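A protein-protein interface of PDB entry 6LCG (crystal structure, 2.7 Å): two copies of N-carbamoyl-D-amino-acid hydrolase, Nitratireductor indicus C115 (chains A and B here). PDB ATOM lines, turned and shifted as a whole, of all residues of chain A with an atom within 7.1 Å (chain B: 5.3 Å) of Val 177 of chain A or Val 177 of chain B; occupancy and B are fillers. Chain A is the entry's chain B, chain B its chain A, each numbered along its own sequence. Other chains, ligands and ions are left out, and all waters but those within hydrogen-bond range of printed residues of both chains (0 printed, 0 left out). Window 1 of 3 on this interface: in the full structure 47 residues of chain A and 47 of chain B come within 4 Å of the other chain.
Printed residues of chain B that touch a printed residue of chain A: Arg 175, Trp 176, Val 177, Glu 178, Arg 181, Val 182 and Gln 225.
Printed residues of chain A that touch a printed residue of chain B: Arg 175, Trp 176, Val 177, Glu 178, Arg 181, Thr 218, Gln 225, Phe 286, Tyr 297 and Ile 300.
Hydrophobic or aromatic side chains of chain A within 4 Å of the printed part of chain B: Trp 176, Val 177, Phe 286, Tyr 297 and Ile 300.
Along chain A the printed residues that touch a printed residue of chain B span positions 175 to 300.
Among the printed residues, 17 pairs touch across the chains.
NH1 of Arg 181 of chain B lies within hydrogen-bond range of O of Gln 225 of chain B (3.4 Å).
OG1 of Thr 218 of chain A sits close to O of Arg 174 of chain A (3.5 Å).
The backbone carbonyl oxygen of Thr 218 of chain A sits at hydrogen-bond distance from the side-chain hydroxyl of Tyr 180 of chain A.
The guanidinium group (NH1) of Arg 181 of chain A sits at hydrogen-bond distance from the backbone carbonyl oxygen (O) of Gln 225 of chain A (3.3 Å).
The side-chain amide oxygen of Asn 226 of chain A sits at hydrogen-bond distance from the guanidinium group of Arg 181 of chain A (2.5 Å).
The backbone carbonyl oxygen (O) of Arg 175 of chain B sits at hydrogen-bond distance from the side-chain amide nitrogen (NE2) of Gln 225 of chain A (3.3 Å).
OE2 of Glu 178 of chain B is in salt-bridge range of NE of Arg 181 of chain A, at 2.7 Å.
The guanidinium group of Arg 181 of chain B lies within salt-bridge range of the side-chain carboxylate of Glu 178 of chain A (2.6 Å).
NE2 of Gln 225 of chain B is in hydrogen-bond range of O of Arg 175 of chain A, at 3.0 Å.
Arg 175 of chain A touches Gln 225 of chain B, and with the chains exchanged Gln 225 of chain A touches Arg 175 of chain B.
Trp 176 of chain A touches Arg 181 of chain B, and with the chains exchanged Arg 181 of chain A touches Trp 176 of chain B.
Val 177 of chain A touches its own counterpart, Val 177 of chain B.
Glu 178 of chain A touches Arg 181 of chain B, and with the chains exchanged Arg 181 of chain A touches Glu 178 of chain B.
9 positions are printed for both chains.
Val 177 of chain A touches just these residues of chain B: Val 177, Arg 181 and Gln 225.
Of chain A, only Val 177, Arg 181 and Gln 225 come within 4 Å of Val 177 of chain B.
Of the printed residues of chain A, Trp 176 of chain B touches Arg 181 (3.4 Å).
Printed residues of chain B within 4 Å of Arg 181 of chain A: Trp 176, Val 177 and Glu 178.
Of the printed residues of chain B, Trp 176 of chain A touches Arg 181.
Thr 179 of chain A touches none of the printed residues of chain B.
The nearest printed residue of chain B that does not touch Val 177 of chain A is Glu 178 of chain B (5.8 Å).
Among the printed residues, merely in contact across the chains: Trp 176 of chain A with Arg 181 of chain B (3.6 Å), Val 177 of chain A with Val 177 of chain B (3.8 Å), Val 177 of chain A with Arg 181 of chain B (3.4 Å), Val 177 of chain A with Gln 225 of chain B (3.3 Å), Arg 181 of chain A with Trp 176 of chain B (3.4 Å), Arg 181 of chain A with Val 177 of chain B (3.4 Å), Thr 218 of chain A with Gln 225 of chain B (3.9 Å), Gln 225 of chain A with Val 177 of chain B (3.3 Å), Phe 286 of chain A with Arg 175 of chain B (3.4 Å), Tyr 297 of chain A with Glu 178 of chain B (3.5 Å), Tyr 297 of chain A with Val 182 of chain B (3.9 Å), Ile 300 of chain A with Glu 178 of chain B (3.7 Å) and Ile 300 of chain A with Arg 181 of chain B (3.9 Å).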
ATOM      1  N   ASP A 173     -28.406 -20.573 -18.201  1.00  0.00           N
ATOM      2  CA  ASP A 173     -26.948 -20.639 -18.268  1.00  0.00           C
ATOM      3  C   ASP A 173     -26.372 -21.114 -16.944  1.00  0.00           C
ATOM      4  O   ASP A 173     -25.290 -21.706 -16.913  1.00  0.00           O
ATOM      5  CB  ASP A 173     -26.345 -19.279 -18.627  1.00  0.00           C
ATOM      6  CG  ASP A 173     -26.592 -18.883 -20.069  1.00  0.00           C
ATOM      7  OD1 ASP A 173     -26.728 -19.777 -20.927  1.00  0.00           O
ATOM      8  OD2 ASP A 173     -26.639 -17.665 -20.345  1.00  0.00           O
ATOM      9  N   ARG A 174     -27.094 -20.879 -15.845  1.00  0.00           N
ATOM     10  CA  ARG A 174     -26.581 -21.160 -14.513  1.00  0.00           C
ATOM     11  C   ARG A 174     -26.530 -22.647 -14.190  1.00  0.00           C
ATOM     12  O   ARG A 174     -25.901 -23.020 -13.195  1.00  0.00           O
ATOM     13  CB  ARG A 174     -27.427 -20.429 -13.468  1.00  0.00           C
ATOM     14  CG  ARG A 174     -28.807 -21.021 -13.238  1.00  0.00           C
ATOM     15  CD  ARG A 174     -29.711 -20.006 -12.558  1.00  0.00           C
ATOM     16  NE  ARG A 174     -30.920 -20.605 -12.001  1.00  0.00           N
ATOM     17  CZ  ARG A 174     -32.053 -20.766 -12.676  1.00  0.00           C
ATOM     18  NH1 ARG A 174     -32.136 -20.380 -13.941  1.00  0.00           N
ATOM     19  NH2 ARG A 174     -33.103 -21.318 -12.084  1.00  0.00           N
ATOM     20  N   ARG A 175     -27.162 -23.503 -14.991  1.00  0.00           N
ATOM     21  CA  ARG A 175     -27.105 -24.939 -14.754  1.00  0.00           C
ATOM     22  C   ARG A 175     -25.946 -25.613 -15.476  1.00  0.00           C
ATOM     23  O   ARG A 175     -25.751 -26.822 -15.310  1.00  0.00           O
ATOM     24  CB  ARG A 175     -28.424 -25.606 -15.164  1.00  0.00           C
ATOM     25  CG  ARG A 175     -28.676 -25.654 -16.661  1.00  0.00           C
ATOM     26  CD  ARG A 175     -29.697 -26.728 -17.004  1.00  0.00           C
ATOM     27  NE  ARG A 175     -30.924 -26.589 -16.225  1.00  0.00           N
ATOM     28  CZ  ARG A 175     -32.059 -26.083 -16.697  1.00  0.00           C
ATOM     29  NH1 ARG A 175     -33.126 -25.996 -15.914  1.00  0.00           N
ATOM     30  NH2 ARG A 175     -32.130 -25.667 -17.954  1.00  0.00           N
ATOM     31  N   TRP A 176     -25.177 -24.870 -16.266  1.00  0.00           N
ATOM     32  CA  TRP A 176     -24.020 -25.405 -16.969  1.00  0.00           C
ATOM     33  C   TRP A 176     -22.746 -24.965 -16.259  1.00  0.00           C
ATOM     34  O   TRP A 176     -22.569 -23.776 -15.975  1.00  0.00           O
ATOM     35  CB  TRP A 176     -24.005 -24.942 -18.426  1.00  0.00           C
ATOM     36  CG  TRP A 176     -25.200 -25.395 -19.202  1.00  0.00           C
ATOM     37  CD1 TRP A 176     -26.290 -24.648 -19.543  1.00  0.00           C
ATOM     38  CD2 TRP A 176     -25.434 -26.707 -19.726  1.00  0.00           C
ATOM     39  NE1 TRP A 176     -27.185 -25.411 -20.251  1.00  0.00           N
ATOM     40  CE2 TRP A 176     -26.684 -26.680 -20.377  1.00  0.00           C
ATOM     41  CE3 TRP A 176     -24.707 -27.902 -19.711  1.00  0.00           C
ATOM     42  CZ2 TRP A 176     -27.222 -27.801 -21.006  1.00  0.00           C
ATOM     43  CZ3 TRP A 176     -25.244 -29.013 -20.335  1.00  0.00           C
ATOM     44  CH2 TRP A 176     -26.489 -28.955 -20.974  1.00  0.00           C
ATOM     45  N   VAL A 177     -21.864 -25.928 -15.975  1.00  0.00           N
ATOM     46  CA  VAL A 177     -20.613 -25.611 -15.297  1.00  0.00           C
ATOM     47  C   VAL A 177     -19.694 -24.774 -16.175  1.00  0.00           C
ATOM     48  O   VAL A 177     -18.811 -24.080 -15.659  1.00  0.00           O
ATOM     49  CB  VAL A 177     -19.897 -26.899 -14.844  1.00  0.00           C
ATOM     50  CG1 VAL A 177     -20.803 -27.728 -13.949  1.00  0.00           C
ATOM     51  CG2 VAL A 177     -19.437 -27.709 -16.047  1.00  0.00           C
ATOM     52  N   GLU A 178     -19.881 -24.819 -17.498  1.00  0.00           N
ATOM     53  CA  GLU A 178     -19.035 -24.034 -18.389  1.00  0.00           C
ATOM     54  C   GLU A 178     -19.307 -22.542 -18.252  1.00  0.00           C
ATOM     55  O   GLU A 178     -18.412 -21.726 -18.497  1.00  0.00           O
ATOM     56  CB  GLU A 178     -19.240 -24.474 -19.840  1.00  0.00           C
ATOM     57  CG  GLU A 178     -18.802 -25.902 -20.150  1.00  0.00           C
ATOM     58  CD  GLU A 178     -19.879 -26.933 -19.860  1.00  0.00           C
ATOM     59  OE1 GLU A 178     -20.850 -26.603 -19.146  1.00  0.00           O
ATOM     60  OE2 GLU A 178     -19.756 -28.075 -20.350  1.00  0.00           O
ATOM     61  N   THR A 179     -20.528 -22.168 -17.863  1.00  0.00           N
ATOM     62  CA  THR A 179     -20.867 -20.756 -17.722  1.00  0.00           C
ATOM     63  C   THR A 179     -20.010 -20.087 -16.655  1.00  0.00           C
ATOM     64  O   THR A 179     -19.465 -18.998 -16.869  1.00  0.00           O
ATOM     65  CB  THR A 179     -22.353 -20.609 -17.392  1.00  0.00           C
ATOM     66  OG1 THR A 179     -23.137 -21.033 -18.513  1.00  0.00           O
ATOM     67  CG2 THR A 179     -22.692 -19.165 -17.055  1.00  0.00           C
ATOM     68  N   TYR A 180     -19.872 -20.733 -15.495  1.00  0.00           N
ATOM     69  CA  TYR A 180     -19.073 -20.151 -14.421  1.00  0.00           C
ATOM     70  C   TYR A 180     -17.582 -20.258 -14.718  1.00  0.00           C
ATOM     71  O   TYR A 180     -16.813 -19.344 -14.396  1.00  0.00           O
ATOM     72  CB  TYR A 180     -19.396 -20.837 -13.093  1.00  0.00           C
ATOM     73  CG  TYR A 180     -20.860 -20.847 -12.722  1.00  0.00           C
ATOM     74  CD1 TYR A 180     -21.430 -19.784 -12.034  1.00  0.00           C
ATOM     75  CD2 TYR A 180     -21.669 -21.930 -13.042  1.00  0.00           C
ATOM     76  CE1 TYR A 180     -22.767 -19.795 -11.685  1.00  0.00           C
ATOM     77  CE2 TYR A 180     -23.006 -21.949 -12.698  1.00  0.00           C
ATOM     78  CZ  TYR A 180     -23.549 -20.879 -12.019  1.00  0.00           C
ATOM     79  OH  TYR A 180     -24.881 -20.894 -11.673  1.00  0.00           O
ATOM     80  N   ARG A 181     -17.153 -21.365 -15.330  1.00  0.00           N
ATOM     81  CA  ARG A 181     -15.724 -21.605 -15.509  1.00  0.00           C
ATOM     82  C   ARG A 181     -15.129 -20.689 -16.574  1.00  0.00           C
ATOM     83  O   ARG A 181     -13.998 -20.212 -16.423  1.00  0.00           O
ATOM     84  CB  ARG A 181     -15.481 -23.074 -15.860  1.00  0.00           C
ATOM     85  CG  ARG A 181     -14.043 -23.400 -16.243  1.00  0.00           C
ATOM     86  CD  ARG A 181     -13.071 -23.197 -15.086  1.00  0.00           C
ATOM     87  NE  ARG A 181     -12.990 -24.363 -14.208  1.00  0.00           N
ATOM     88  CZ  ARG A 181     -13.417 -24.388 -12.950  1.00  0.00           C
ATOM     89  NH1 ARG A 181     -13.956 -23.304 -12.409  1.00  0.00           N
ATOM     90  NH2 ARG A 181     -13.300 -25.497 -12.230  1.00  0.00           N
ATOM     91  N   VAL A 182     -15.870 -20.432 -17.656  1.00  0.00           N
ATOM     92  CA  VAL A 182     -15.365 -19.554 -18.709  1.00  0.00           C
ATOM     93  C   VAL A 182     -15.109 -18.155 -18.161  1.00  0.00           C
ATOM     94  O   VAL A 182     -14.078 -17.536 -18.453  1.00  0.00           O
ATOM     95  CB  VAL A 182     -16.338 -19.529 -19.903  1.00  0.00           C
ATOM     96  CG1 VAL A 182     -16.009 -18.375 -20.838  1.00  0.00           C
ATOM     97  CG2 VAL A 182     -16.278 -20.847 -20.658  1.00  0.00           C
ATOM     98  N   THR A 218     -26.784 -25.267  -8.245  1.00  0.00           N
ATOM     99  CA  THR A 218     -25.939 -24.876  -9.369  1.00  0.00           C
ATOM    100  C   THR A 218     -25.241 -23.548  -9.104  1.00  0.00           C
ATOM    101  O   THR A 218     -24.098 -23.346  -9.530  1.00  0.00           O
ATOM    102  CB  THR A 218     -26.767 -24.794 -10.652  1.00  0.00           C
ATOM    103  OG1 THR A 218     -27.854 -23.878 -10.465  1.00  0.00           O
ATOM    104  CG2 THR A 218     -27.314 -26.162 -11.026  1.00  0.00           C
ATOM    105  N   ALA A 221     -22.527 -23.899  -6.228  1.00  0.00           N
ATOM    106  CA  ALA A 221     -21.341 -24.591  -6.716  1.00  0.00           C
ATOM    107  C   ALA A 221     -20.521 -23.699  -7.639  1.00  0.00           C
ATOM    108  O   ALA A 221     -19.293 -23.630  -7.519  1.00  0.00           O
ATOM    109  CB  ALA A 221     -21.741 -25.878  -7.433  1.00  0.00           C
ATOM    110  N   GLY A 222     -21.185 -23.010  -8.570  1.00  0.00           N
ATOM    111  CA  GLY A 222     -20.473 -22.107  -9.458  1.00  0.00           C
ATOM    112  C   GLY A 222     -19.792 -20.972  -8.723  1.00  0.00           C
ATOM    113  O   GLY A 222     -18.757 -20.468  -9.171  1.00  0.00           O
ATOM    114  N   GLN A 225     -16.747 -23.058  -6.624  1.00  0.00           N
ATOM    115  CA  GLN A 225     -15.748 -23.674  -7.490  1.00  0.00           C
ATOM    116  C   GLN A 225     -15.044 -22.672  -8.396  1.00  0.00           C
ATOM    117  O   GLN A 225     -14.104 -23.057  -9.100  1.00  0.00           O
ATOM    118  CB  GLN A 225     -16.396 -24.777  -8.326  1.00  0.00           C
ATOM    119  CG  GLN A 225     -16.966 -25.906  -7.485  1.00  0.00           C
ATOM    120  CD  GLN A 225     -17.540 -27.028  -8.321  1.00  0.00           C
ATOM    121  OE1 GLN A 225     -18.674 -26.949  -8.794  1.00  0.00           O
ATOM    122  NE2 GLN A 225     -16.757 -28.083  -8.510  1.00  0.00           N
ATOM    123  N   ASN A 226     -15.470 -21.410  -8.396  1.00  0.00           N
ATOM    124  CA  ASN A 226     -14.776 -20.353  -9.115  1.00  0.00           C
ATOM    125  C   ASN A 226     -14.399 -19.182  -8.220  1.00  0.00           C
ATOM    126  O   ASN A 226     -13.819 -18.208  -8.714  1.00  0.00           O
ATOM    127  CB  ASN A 226     -15.630 -19.851 -10.287  1.00  0.00           C
ATOM    128  CG  ASN A 226     -15.860 -20.917 -11.335  1.00  0.00           C
ATOM    129  OD1 ASN A 226     -15.095 -21.040 -12.291  1.00  0.00           O
ATOM    130  ND2 ASN A 226     -16.915 -21.702 -11.157  1.00  0.00           N
ATOM    131  N   PHE A 286      -8.299 -22.733  -5.424  1.00  0.00           N
ATOM    132  CA  PHE A 286      -8.718 -22.661  -6.819  1.00  0.00           C
ATOM    133  C   PHE A 286      -7.775 -21.790  -7.643  1.00  0.00           C
ATOM    134  O   PHE A 286      -8.208 -20.959  -8.444  1.00  0.00           O
ATOM    135  CB  PHE A 286     -10.154 -22.159  -6.929  1.00  0.00           C
ATOM    136  CG  PHE A 286     -11.171 -23.123  -6.388  1.00  0.00           C
ATOM    137  CD1 PHE A 286     -11.495 -24.272  -7.090  1.00  0.00           C
ATOM    138  CD2 PHE A 286     -11.800 -22.882  -5.177  1.00  0.00           C
ATOM    139  CE1 PHE A 286     -12.428 -25.163  -6.597  1.00  0.00           C
ATOM    140  CE2 PHE A 286     -12.735 -23.770  -4.679  1.00  0.00           C
ATOM    141  CZ  PHE A 286     -13.049 -24.912  -5.390  1.00  0.00           C
ATOM    142  N   TYR A 297      -8.789 -31.893 -20.492  1.00  0.00           N
ATOM    143  CA  TYR A 297     -10.134 -31.347 -20.612  1.00  0.00           C
ATOM    144  C   TYR A 297     -10.587 -31.222 -22.062  1.00  0.00           C
ATOM    145  O   TYR A 297     -11.592 -30.556 -22.329  1.00  0.00           O
ATOM    146  CB  TYR A 297     -10.219 -29.974 -19.936  1.00  0.00           C
ATOM    147  CG  TYR A 297      -9.657 -29.891 -18.529  1.00  0.00           C
ATOM    148  CD1 TYR A 297      -9.591 -31.008 -17.705  1.00  0.00           C
ATOM    149  CD2 TYR A 297      -9.202 -28.678 -18.023  1.00  0.00           C
ATOM    150  CE1 TYR A 297      -9.076 -30.920 -16.423  1.00  0.00           C
ATOM    151  CE2 TYR A 297      -8.688 -28.582 -16.746  1.00  0.00           C
ATOM    152  CZ  TYR A 297      -8.628 -29.704 -15.949  1.00  0.00           C
ATOM    153  OH  TYR A 297      -8.117 -29.605 -14.675  1.00  0.00           O
ATOM    154  N   ILE A 300     -14.208 -31.255 -23.515  1.00  0.00           N
ATOM    155  CA  ILE A 300     -15.154 -30.180 -23.225  1.00  0.00           C
ATOM    156  C   ILE A 300     -15.357 -29.294 -24.449  1.00  0.00           C
ATOM    157  O   ILE A 300     -16.463 -28.796 -24.695  1.00  0.00           O
ATOM    158  CB  ILE A 300     -14.678 -29.372 -22.003  1.00  0.00           C
ATOM    159  CG1 ILE A 300     -14.651 -30.262 -20.759  1.00  0.00           C
ATOM    160  CG2 ILE A 300     -15.569 -28.159 -21.768  1.00  0.00           C
ATOM    161  CD1 ILE A 300     -14.186 -29.556 -19.510  1.00  0.00           C
ATOM    162  N   ARG B 175     -13.227 -31.501  -6.720  1.00  0.00           N
ATOM    163  CA  ARG B 175     -13.390 -30.060  -6.587  1.00  0.00           C
ATOM    164  C   ARG B 175     -13.342 -29.329  -7.922  1.00  0.00           C
ATOM    165  O   ARG B 175     -13.553 -28.113  -7.954  1.00  0.00           O
ATOM    166  CB  ARG B 175     -12.317 -29.498  -5.651  1.00  0.00           C
ATOM    167  CG  ARG B 175     -12.596 -29.739  -4.177  1.00  0.00           C
ATOM    168  CD  ARG B 175     -11.309 -29.825  -3.379  1.00  0.00           C
ATOM    169  NE  ARG B 175     -10.352 -28.797  -3.771  1.00  0.00           N
ATOM    170  CZ  ARG B 175      -9.138 -28.666  -3.244  1.00  0.00           C
ATOM    171  NH1 ARG B 175      -8.732 -29.500  -2.296  1.00  0.00           N
ATOM    172  NH2 ARG B 175      -8.332 -27.702  -3.664  1.00  0.00           N
ATOM    173  N   TRP B 176     -13.079 -30.036  -9.018  1.00  0.00           N
ATOM    174  CA  TRP B 176     -12.996 -29.442 -10.346  1.00  0.00           C
ATOM    175  C   TRP B 176     -14.188 -29.888 -11.181  1.00  0.00           C
ATOM    176  O   TRP B 176     -14.479 -31.085 -11.267  1.00  0.00           O
ATOM    177  CB  TRP B 176     -11.689 -29.834 -11.039  1.00  0.00           C
ATOM    178  CG  TRP B 176     -10.475 -29.332 -10.329  1.00  0.00           C
ATOM    179  CD1 TRP B 176      -9.637 -30.048  -9.526  1.00  0.00           C
ATOM    180  CD2 TRP B 176      -9.966 -27.994 -10.349  1.00  0.00           C
ATOM    181  NE1 TRP B 176      -8.635 -29.241  -9.048  1.00  0.00           N
ATOM    182  CE2 TRP B 176      -8.814 -27.974  -9.539  1.00  0.00           C
ATOM    183  CE3 TRP B 176     -10.372 -26.812 -10.974  1.00  0.00           C
ATOM    184  CZ2 TRP B 176      -8.064 -26.818  -9.338  1.00  0.00           C
ATOM    185  CZ3 TRP B 176      -9.625 -25.665 -10.773  1.00  0.00           C
ATOM    186  CH2 TRP B 176      -8.484 -25.676  -9.962  1.00  0.00           C
ATOM    187  N   VAL B 177     -14.872 -28.919 -11.799  1.00  0.00           N
ATOM    188  CA  VAL B 177     -16.013 -29.238 -12.648  1.00  0.00           C
ATOM    189  C   VAL B 177     -15.586 -29.988 -13.902  1.00  0.00           C
ATOM    190  O   VAL B 177     -16.399 -30.708 -14.495  1.00  0.00           O
ATOM    191  CB  VAL B 177     -16.787 -27.959 -13.024  1.00  0.00           C
ATOM    192  CG1 VAL B 177     -17.301 -27.263 -11.774  1.00  0.00           C
ATOM    193  CG2 VAL B 177     -15.909 -27.022 -13.840  1.00  0.00           C
ATOM    194  N   GLU B 178     -14.327 -29.841 -14.321  1.00  0.00           N
ATOM    195  CA  GLU B 178     -13.849 -30.559 -15.497  1.00  0.00           C
ATOM    196  C   GLU B 178     -13.775 -32.058 -15.244  1.00  0.00           C
ATOM    197  O   GLU B 178     -13.892 -32.849 -16.187  1.00  0.00           O
ATOM    198  CB  GLU B 178     -12.478 -30.030 -15.920  1.00  0.00           C
ATOM    199  CG  GLU B 178     -12.455 -28.568 -16.348  1.00  0.00           C
ATOM    200  CD  GLU B 178     -12.245 -27.608 -15.189  1.00  0.00           C
ATOM    201  OE1 GLU B 178     -12.484 -28.001 -14.028  1.00  0.00           O
ATOM    202  OE2 GLU B 178     -11.834 -26.456 -15.442  1.00  0.00           O
ATOM    203  N   THR B 179     -13.577 -32.465 -13.989  1.00  0.00           N
ATOM    204  CA  THR B 179     -13.525 -33.888 -13.665  1.00  0.00           C
ATOM    205  C   THR B 179     -14.842 -34.575 -14.001  1.00  0.00           C
ATOM    206  O   THR B 179     -14.859 -35.637 -14.634  1.00  0.00           O
ATOM    207  CB  THR B 179     -13.185 -34.072 -12.185  1.00  0.00           C
ATOM    208  OG1 THR B 179     -11.849 -33.615 -11.938  1.00  0.00           O
ATOM    209  CG2 THR B 179     -13.305 -35.535 -11.782  1.00  0.00           C
ATOM    210  N   TYR B 180     -15.962 -33.976 -13.591  1.00  0.00           N
ATOM    211  CA  TYR B 180     -17.263 -34.583 -13.853  1.00  0.00           C
ATOM    212  C   TYR B 180     -17.655 -34.446 -15.319  1.00  0.00           C
ATOM    213  O   TYR B 180     -18.201 -35.384 -15.911  1.00  0.00           O
ATOM    214  CB  TYR B 180     -18.331 -33.949 -12.963  1.00  0.00           C
ATOM    215  CG  TYR B 180     -18.016 -33.955 -11.485  1.00  0.00           C
ATOM    216  CD1 TYR B 180     -17.321 -32.903 -10.900  1.00  0.00           C
ATOM    217  CD2 TYR B 180     -18.430 -35.001 -10.670  1.00  0.00           C
ATOM    218  CE1 TYR B 180     -17.038 -32.899  -9.550  1.00  0.00           C
ATOM    219  CE2 TYR B 180     -18.151 -35.004  -9.317  1.00  0.00           C
ATOM    220  CZ  TYR B 180     -17.454 -33.950  -8.763  1.00  0.00           C
ATOM    221  OH  TYR B 180     -17.177 -33.948  -7.417  1.00  0.00           O
ATOM    222  N   ARG B 181     -17.385 -33.285 -15.920  1.00  0.00           N
ATOM    223  CA  ARG B 181     -17.858 -33.023 -17.277  1.00  0.00           C
ATOM    224  C   ARG B 181     -17.148 -33.903 -18.300  1.00  0.00           C
ATOM    225  O   ARG B 181     -17.776 -34.385 -19.249  1.00  0.00           O
ATOM    226  CB  ARG B 181     -17.678 -31.542 -17.616  1.00  0.00           C
ATOM    227  CG  ARG B 181     -18.010 -31.184 -19.057  1.00  0.00           C
ATOM    228  CD  ARG B 181     -19.482 -31.397 -19.387  1.00  0.00           C
ATOM    229  NE  ARG B 181     -20.313 -30.248 -19.030  1.00  0.00           N
ATOM    230  CZ  ARG B 181     -21.210 -30.242 -18.049  1.00  0.00           C
ATOM    231  NH1 ARG B 181     -21.404 -31.330 -17.318  1.00  0.00           N
ATOM    232  NH2 ARG B 181     -21.918 -29.148 -17.803  1.00  0.00           N
ATOM    233  N   VAL B 182     -15.842 -34.128 -18.124  1.00  0.00           N
ATOM    234  CA  VAL B 182     -15.096 -34.957 -19.069  1.00  0.00           C
ATOM    235  C   VAL B 182     -15.659 -36.374 -19.093  1.00  0.00           C
ATOM    236  O   VAL B 182     -15.867 -36.961 -20.163  1.00  0.00           O
ATOM    237  CB  VAL B 182     -13.595 -34.948 -18.725  1.00  0.00           C
ATOM    238  CG1 VAL B 182     -12.877 -36.082 -19.440  1.00  0.00           C
ATOM    239  CG2 VAL B 182     -12.978 -33.612 -19.104  1.00  0.00           C
ATOM    240  N   GLN B 225     -25.417 -31.934 -12.270  1.00  0.00           N
ATOM    241  CA  GLN B 225     -25.104 -31.257 -13.523  1.00  0.00           C
ATOM    242  C   GLN B 225     -24.547 -32.198 -14.583  1.00  0.00           C
ATOM    243  O   GLN B 225     -24.325 -31.761 -15.717  1.00  0.00           O
ATOM    244  CB  GLN B 225     -24.127 -30.109 -13.265  1.00  0.00           C
ATOM    245  CG  GLN B 225     -24.690 -29.036 -12.344  1.00  0.00           C
ATOM    246  CD  GLN B 225     -23.746 -27.868 -12.148  1.00  0.00           C
ATOM    247  OE1 GLN B 225     -22.807 -27.941 -11.356  1.00  0.00           O
ATOM    248  NE2 GLN B 225     -23.991 -26.781 -12.871  1.00  0.00           N
